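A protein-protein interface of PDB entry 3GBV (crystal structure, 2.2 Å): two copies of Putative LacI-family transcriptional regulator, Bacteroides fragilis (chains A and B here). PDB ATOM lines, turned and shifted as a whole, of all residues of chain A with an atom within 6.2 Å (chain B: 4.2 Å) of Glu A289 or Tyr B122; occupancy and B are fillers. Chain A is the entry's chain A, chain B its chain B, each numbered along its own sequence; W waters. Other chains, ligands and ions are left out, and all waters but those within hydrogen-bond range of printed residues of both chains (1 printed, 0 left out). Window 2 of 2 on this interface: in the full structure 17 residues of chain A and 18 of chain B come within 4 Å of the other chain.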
ATOM      1  N   THR A 287      -8.074  25.488   4.433  1.00  0.00           N
ATOM      2  CA  THR A 287      -6.679  25.084   4.556  1.00  0.00           C
ATOM      3  C   THR A 287      -5.959  26.223   5.259  1.00  0.00           C
ATOM      4  O   THR A 287      -6.531  27.285   5.486  1.00  0.00           O
ATOM      5  CB  THR A 287      -6.010  24.863   3.180  1.00  0.00           C
ATOM      6  OG1 THR A 287      -5.798  26.124   2.537  1.00  0.00           O
ATOM      7  CG2 THR A 287      -6.882  24.011   2.299  1.00  0.00           C
ATOM      8  N   LYS A 288      -4.701  25.996   5.596  1.00  0.00           N
ATOM      9  CA  LYS A 288      -3.902  27.007   6.262  1.00  0.00           C
ATOM     10  C   LYS A 288      -3.844  28.269   5.403  1.00  0.00           C
ATOM     11  O   LYS A 288      -3.863  29.380   5.922  1.00  0.00           O
ATOM     12  CB  LYS A 288      -2.488  26.461   6.486  1.00  0.00           C
ATOM     13  CG  LYS A 288      -1.522  27.380   7.208  1.00  0.00           C
ATOM     14  CD  LYS A 288      -0.143  26.712   7.314  1.00  0.00           C
ATOM     15  CE  LYS A 288       0.957  27.687   7.753  1.00  0.00           C
ATOM     16  NZ  LYS A 288       0.687  28.270   9.101  1.00  0.00           N
ATOM     17  N   GLU A 289      -3.800  28.085   4.086  1.00  0.00           N
ATOM     18  CA  GLU A 289      -3.693  29.199   3.159  1.00  0.00           C
ATOM     19  C   GLU A 289      -4.943  30.037   2.882  1.00  0.00           C
ATOM     20  O   GLU A 289      -4.840  31.078   2.236  1.00  0.00           O
ATOM     21  CB  GLU A 289      -3.130  28.722   1.820  1.00  0.00           C
ATOM     22  CG  GLU A 289      -1.696  28.211   1.849  1.00  0.00           C
ATOM     23  CD  GLU A 289      -1.583  26.836   2.461  1.00  0.00           C
ATOM     24  OE1 GLU A 289      -2.514  26.026   2.259  1.00  0.00           O
ATOM     25  OE2 GLU A 289      -0.562  26.564   3.132  1.00  0.00           O
ATOM     26  N   ASN A 290      -6.118  29.600   3.329  1.00  0.00           N
ATOM     27  CA  ASN A 290      -7.314  30.403   3.089  1.00  0.00           C
ATOM     28  C   ASN A 290      -8.161  30.623   4.341  1.00  0.00           C
ATOM     29  O   ASN A 290      -9.135  31.383   4.317  1.00  0.00           O
ATOM     30  CB  ASN A 290      -8.177  29.790   1.970  1.00  0.00           C
ATOM     31  CG  ASN A 290      -8.961  28.554   2.415  1.00  0.00           C
ATOM     32  OD1 ASN A 290      -9.918  28.147   1.741  1.00  0.00           O
ATOM     33  ND2 ASN A 290      -8.561  27.948   3.533  1.00  0.00           N
ATOM     34  N   ILE A 291      -7.767  29.983   5.441  1.00  0.00           N
ATOM     35  CA  ILE A 291      -8.514  30.103   6.680  1.00  0.00           C
ATOM     36  C   ILE A 291      -8.697  31.536   7.166  1.00  0.00           C
ATOM     37  O   ILE A 291      -9.761  31.868   7.680  1.00  0.00           O
ATOM     38  CB  ILE A 291      -7.880  29.260   7.832  1.00  0.00           C
ATOM     39  CG1 ILE A 291      -8.785  29.293   9.063  1.00  0.00           C
ATOM     40  CG2 ILE A 291      -6.539  29.829   8.241  1.00  0.00           C
ATOM     41  CD1 ILE A 291     -10.160  28.705   8.840  1.00  0.00           C
ATOM     42  N   ASP A 292      -7.689  32.391   6.998  1.00  0.00           N
ATOM     43  CA  ASP A 292      -7.812  33.770   7.479  1.00  0.00           C
ATOM     44  C   ASP A 292      -8.745  34.669   6.661  1.00  0.00           C
ATOM     45  O   ASP A 292      -9.115  35.759   7.101  1.00  0.00           O
ATOM     46  CB  ASP A 292      -6.428  34.427   7.598  1.00  0.00           C
ATOM     47  CG  ASP A 292      -5.494  33.672   8.551  1.00  0.00           C
ATOM     48  OD1 ASP A 292      -5.980  33.064   9.535  1.00  0.00           O
ATOM     49  OD2 ASP A 292      -4.267  33.695   8.320  1.00  0.00           O
ATOM     50  N   TYR A 293      -9.150  34.208   5.486  1.00  0.00           N
ATOM     51  CA  TYR A 293     -10.024  34.998   4.637  1.00  0.00           C
ATOM     52  C   TYR A 293     -11.457  34.471   4.571  1.00  0.00           C
ATOM     53  O   TYR A 293     -12.290  34.993   3.832  1.00  0.00           O
ATOM     54  CB  TYR A 293      -9.404  35.080   3.250  1.00  0.00           C
ATOM     55  CG  TYR A 293      -8.080  35.787   3.295  1.00  0.00           C
ATOM     56  CD1 TYR A 293      -8.023  37.182   3.328  1.00  0.00           C
ATOM     57  CD2 TYR A 293      -6.881  35.068   3.388  1.00  0.00           C
ATOM     58  CE1 TYR A 293      -6.819  37.845   3.454  1.00  0.00           C
ATOM     59  CE2 TYR A 293      -5.658  35.729   3.519  1.00  0.00           C
ATOM     60  CZ  TYR A 293      -5.636  37.115   3.549  1.00  0.00           C
ATOM     61  OH  TYR A 293      -4.443  37.788   3.655  1.00  0.00           O
ATOM     62  N   HIS B 118      -2.295  37.871  -3.834  1.00  0.00           N
ATOM     63  CA  HIS B 118      -1.107  37.077  -3.547  1.00  0.00           C
ATOM     64  C   HIS B 118      -1.441  35.820  -2.766  1.00  0.00           C
ATOM     65  O   HIS B 118      -0.985  34.734  -3.114  1.00  0.00           O
ATOM     66  CB  HIS B 118      -0.080  37.925  -2.794  1.00  0.00           C
ATOM     67  CG  HIS B 118       0.656  38.890  -3.670  1.00  0.00           C
ATOM     68  ND1 HIS B 118       1.777  38.536  -4.392  1.00  0.00           N
ATOM     69  CD2 HIS B 118       0.402  40.183  -3.981  1.00  0.00           C
ATOM     70  CE1 HIS B 118       2.182  39.569  -5.108  1.00  0.00           C
ATOM     71  NE2 HIS B 118       1.364  40.582  -4.878  1.00  0.00           N
ATOM     72  N   GLN B 119      -2.245  35.968  -1.719  1.00  0.00           N
ATOM     73  CA  GLN B 119      -2.643  34.830  -0.904  1.00  0.00           C
ATOM     74  C   GLN B 119      -3.433  33.841  -1.769  1.00  0.00           C
ATOM     75  O   GLN B 119      -3.254  32.630  -1.654  1.00  0.00           O
ATOM     76  CB  GLN B 119      -3.490  35.306   0.278  1.00  0.00           C
ATOM     77  CG  GLN B 119      -3.732  34.243   1.337  1.00  0.00           C
ATOM     78  CD  GLN B 119      -2.437  33.744   1.949  1.00  0.00           C
ATOM     79  OE1 GLN B 119      -1.480  34.512   2.118  1.00  0.00           O
ATOM     80  NE2 GLN B 119      -2.401  32.458   2.293  1.00  0.00           N
ATOM     81  N   SER B 120      -4.295  34.372  -2.638  1.00  0.00           N
ATOM     82  CA  SER B 120      -5.097  33.547  -3.539  1.00  0.00           C
ATOM     83  C   SER B 120      -4.162  32.677  -4.392  1.00  0.00           C
ATOM     84  O   SER B 120      -4.374  31.469  -4.529  1.00  0.00           O
ATOM     85  CB  SER B 120      -5.958  34.435  -4.447  1.00  0.00           C
ATOM     86  OG  SER B 120      -6.805  33.668  -5.277  1.00  0.00           O
ATOM     87  N   GLY B 121      -3.124  33.298  -4.947  1.00  0.00           N
ATOM     88  CA  GLY B 121      -2.162  32.572  -5.762  1.00  0.00           C
ATOM     89  C   GLY B 121      -1.374  31.537  -4.973  1.00  0.00           C
ATOM     90  O   GLY B 121      -1.127  30.435  -5.464  1.00  0.00           O
ATOM     91  N   TYR B 122      -0.979  31.895  -3.755  1.00  0.00           N
ATOM     92  CA  TYR B 122      -0.228  31.004  -2.868  1.00  0.00           C
ATOM     93  C   TYR B 122      -1.079  29.748  -2.616  1.00  0.00           C
ATOM     94  O   TYR B 122      -0.606  28.607  -2.721  1.00  0.00           O
ATOM     95  CB  TYR B 122       0.023  31.722  -1.545  1.00  0.00           C
ATOM     96  CG  TYR B 122       1.159  31.177  -0.715  1.00  0.00           C
ATOM     97  CD1 TYR B 122       2.484  31.338  -1.119  1.00  0.00           C
ATOM     98  CD2 TYR B 122       0.916  30.539   0.501  1.00  0.00           C
ATOM     99  CE1 TYR B 122       3.542  30.880  -0.328  1.00  0.00           C
ATOM    100  CE2 TYR B 122       1.965  30.076   1.301  1.00  0.00           C
ATOM    101  CZ  TYR B 122       3.278  30.253   0.878  1.00  0.00           C
ATOM    102  OH  TYR B 122       4.320  29.813   1.663  1.00  0.00           O
ATOM    103  N   PHE B 123      -2.340  29.991  -2.262  1.00  0.00           N
ATOM    104  CA  PHE B 123      -3.303  28.936  -1.996  1.00  0.00           C
ATOM    105  C   PHE B 123      -3.435  28.013  -3.214  1.00  0.00           C
ATOM    106  O   PHE B 123      -3.394  26.790  -3.074  1.00  0.00           O
ATOM    107  CB  PHE B 123      -4.673  29.540  -1.670  1.00  0.00           C
ATOM    108  CG  PHE B 123      -5.786  28.528  -1.615  1.00  0.00           C
ATOM    109  CD1 PHE B 123      -6.080  27.855  -0.438  1.00  0.00           C
ATOM    110  CD2 PHE B 123      -6.528  28.229  -2.755  1.00  0.00           C
ATOM    111  CE1 PHE B 123      -7.096  26.903  -0.400  1.00  0.00           C
ATOM    112  CE2 PHE B 123      -7.543  27.280  -2.722  1.00  0.00           C
ATOM    113  CZ  PHE B 123      -7.829  26.620  -1.549  1.00  0.00           C
ATOM    114  N   ALA B 124      -3.601  28.609  -4.394  1.00  0.00           N
ATOM    115  CA  ALA B 124      -3.745  27.856  -5.642  1.00  0.00           C
ATOM    116  C   ALA B 124      -2.568  26.914  -5.874  1.00  0.00           C
ATOM    117  O   ALA B 124      -2.742  25.778  -6.318  1.00  0.00           O
ATOM    118  CB  ALA B 124      -3.878  28.812  -6.817  1.00  0.00           C
ATOM    119  N   ALA B 125      -1.369  27.402  -5.585  1.00  0.00           N
ATOM    120  CA  ALA B 125      -0.162  26.603  -5.748  1.00  0.00           C
ATOM    121  C   ALA B 125      -0.215  25.391  -4.828  1.00  0.00           C
ATOM    122  O   ALA B 125       0.070  24.272  -5.254  1.00  0.00           O
ATOM    123  CB  ALA B 125       1.048  27.435  -5.419  1.00  0.00           C
ATOM    124  N   ARG B 126      -0.567  25.631  -3.562  1.00  0.00           N
ATOM    125  CA  ARG B 126      -0.665  24.570  -2.561  1.00  0.00           C
ATOM    126  C   ARG B 126      -1.600  23.471  -3.027  1.00  0.00           C
ATOM    127  O   ARG B 126      -1.294  22.286  -2.884  1.00  0.00           O
ATOM    128  CB  ARG B 126      -1.170  25.141  -1.228  1.00  0.00           C
ATOM    129  CG  ARG B 126      -1.901  24.147  -0.313  1.00  0.00           C
ATOM    130  CD  ARG B 126      -1.023  23.014   0.162  1.00  0.00           C
ATOM    131  NE  ARG B 126      -1.759  22.065   1.000  1.00  0.00           N
ATOM    132  CZ  ARG B 126      -2.141  22.302   2.254  1.00  0.00           C
ATOM    133  NH1 ARG B 126      -1.864  23.462   2.832  1.00  0.00           N
ATOM    134  NH2 ARG B 126      -2.793  21.369   2.938  1.00  0.00           N
ATOM    135  N   GLY B 160       2.104  35.415  -6.418  1.00  0.00           N
ATOM    136  CA  GLY B 160       1.965  34.693  -5.164  1.00  0.00           C
ATOM    137  C   GLY B 160       2.182  33.218  -5.442  1.00  0.00           C
ATOM    138  O   GLY B 160       2.837  32.513  -4.672  1.00  0.00           O
ATOM    139  N   PHE B 161       1.626  32.755  -6.558  1.00  0.00           N
ATOM    140  CA  PHE B 161       1.762  31.363  -6.965  1.00  0.00           C
ATOM    141  C   PHE B 161       3.257  31.032  -7.080  1.00  0.00           C
ATOM    142  O   PHE B 161       3.756  30.105  -6.434  1.00  0.00           O
ATOM    143  CB  PHE B 161       1.084  31.153  -8.321  1.00  0.00           C
ATOM    144  CG  PHE B 161       1.231  29.751  -8.880  1.00  0.00           C
ATOM    145  CD1 PHE B 161       0.323  28.755  -8.541  1.00  0.00           C
ATOM    146  CD2 PHE B 161       2.267  29.440  -9.768  1.00  0.00           C
ATOM    147  CE1 PHE B 161       0.432  27.481  -9.066  1.00  0.00           C
ATOM    148  CE2 PHE B 161       2.389  28.167 -10.301  1.00  0.00           C
ATOM    149  CZ  PHE B 161       1.464  27.180  -9.952  1.00  0.00           C
ATOM    150  N   TYR B 164       5.181  30.658  -3.855  1.00  0.00           N
ATOM    151  CA  TYR B 164       4.961  29.394  -3.170  1.00  0.00           C
ATOM    152  C   TYR B 164       5.807  28.314  -3.831  1.00  0.00           C
ATOM    153  O   TYR B 164       6.444  27.516  -3.153  1.00  0.00           O
ATOM    154  CB  TYR B 164       3.490  28.964  -3.257  1.00  0.00           C
ATOM    155  CG  TYR B 164       3.194  27.661  -2.534  1.00  0.00           C
ATOM    156  CD1 TYR B 164       2.668  27.657  -1.238  1.00  0.00           C
ATOM    157  CD2 TYR B 164       3.451  26.435  -3.141  1.00  0.00           C
ATOM    158  CE1 TYR B 164       2.406  26.450  -0.565  1.00  0.00           C
ATOM    159  CE2 TYR B 164       3.200  25.233  -2.482  1.00  0.00           C
ATOM    160  CZ  TYR B 164       2.677  25.244  -1.199  1.00  0.00           C
ATOM    161  OH  TYR B 164       2.451  24.046  -0.556  1.00  0.00           O
ATOM    162  N   GLU B 167       9.357  28.517  -3.123  1.00  0.00           N
ATOM    163  CA  GLU B 167       9.470  28.259  -1.695  1.00  0.00           C
ATOM    164  C   GLU B 167       9.329  26.800  -1.232  1.00  0.00           C
ATOM    165  O   GLU B 167       9.974  26.392  -0.266  1.00  0.00           O
ATOM    166  CB  GLU B 167       8.427  29.124  -0.992  1.00  0.00           C
ATOM    167  CG  GLU B 167       8.709  29.486   0.441  1.00  0.00           C
ATOM    168  CD  GLU B 167       7.629  30.403   0.996  1.00  0.00           C
ATOM    169  OE1 GLU B 167       7.554  31.579   0.570  1.00  0.00           O
ATOM    170  OE2 GLU B 167       6.841  29.938   1.848  1.00  0.00           O
ATOM    171  N   HIS B 168       8.495  26.022  -1.915  1.00  0.00           N
ATOM    172  CA  HIS B 168       8.258  24.632  -1.532  1.00  0.00           C
ATOM    173  C   HIS B 168       8.636  23.609  -2.591  1.00  0.00           C
ATOM    174  O   HIS B 168       8.933  22.462  -2.260  1.00  0.00           O
ATOM    175  CB  HIS B 168       6.782  24.434  -1.179  1.00  0.00           C
ATOM    176  CG  HIS B 168       6.307  25.292  -0.048  1.00  0.00           C
ATOM    177  ND1 HIS B 168       6.617  25.028   1.269  1.00  0.00           N
ATOM    178  CD2 HIS B 168       5.552  26.413  -0.040  1.00  0.00           C
ATOM    179  CE1 HIS B 168       6.070  25.950   2.040  1.00  0.00           C
ATOM    180  NE2 HIS B 168       5.418  26.803   1.271  1.00  0.00           N
HETATM  181  O   HOH W   1      -3.859  23.287   5.406  1.00  0.00           O
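Among the printed residues, pairs that only touch across the chains: Tyr A293 with Gln B119 (3.3 Å), Thr A287 with Phe B123 (3.3 Å), Asn A290 with Phe B123 (3.7 Å), Glu A289 with Tyr B122 (3.7 Å) and Glu A289 with Phe B123 (3.8 Å).
No position is printed for both chains.
The guanidinium group of Arg B126 is in salt-bridge range of the side-chain carboxylate of Glu A289.
The backbone carbonyl oxygen of Glu A289 lies within hydrogen-bond range of the side-chain amide nitrogen of Gln B119 (2.8 Å).
The side-chain hydroxyl (OG1) of Thr A287 sits close to the backbone NH (N) of Glu A289, at 3.2 Å.
The side-chain hydroxyl of Tyr B122 lies within hydrogen-bond range of the side-chain carboxylate of Glu B167 (2.5 Å).
N of Thr A287 sits close to ND2 of Asn A290 (2.7 Å).
OH of Tyr B122 lies within hydrogen-bond range of NE2 of His B168, at 3.2 Å.
Of the 7 printed residues of chain A, 4 touch a printed residue of chain B.
Hydrophobic or aromatic side chains of chain B within 4 Å of the printed part of chain A: Tyr B122 and Phe B123.
Among the printed residues, Asp or Glu carboxylates within 4 Å of a Lys or Arg side-chain nitrogen of the other chain: Glu A289 with Arg B126 (2.7 Å).
Of chain B, only Gln B119 (2.8 Å), Tyr B122 (3.7 Å), Phe B123 (3.8 Å) and Arg B126 (2.7 Å) come within 4 Å of Glu A289.
Of chain A, only Glu A289 comes within 4 Å of Tyr B122.
Of the printed residues of chain B, Tyr A293 touches Gln B119 (3.3 Å).
Of the printed residues of chain B, Thr A287 touches Phe B123.
Of the printed residues of chain A, Phe B123 touches Thr A287, Glu A289 and Asn A290.
His B118 touches none of the printed residues of chain A.
His B168 touches none of the printed residues of chain A.
The nearest printed residue of chain A that does not touch Tyr B122 is Lys A288 (7.0 Å).
Water W1 lies within hydrogen-bond range of N of Lys A288 and NH1 of Arg B126.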
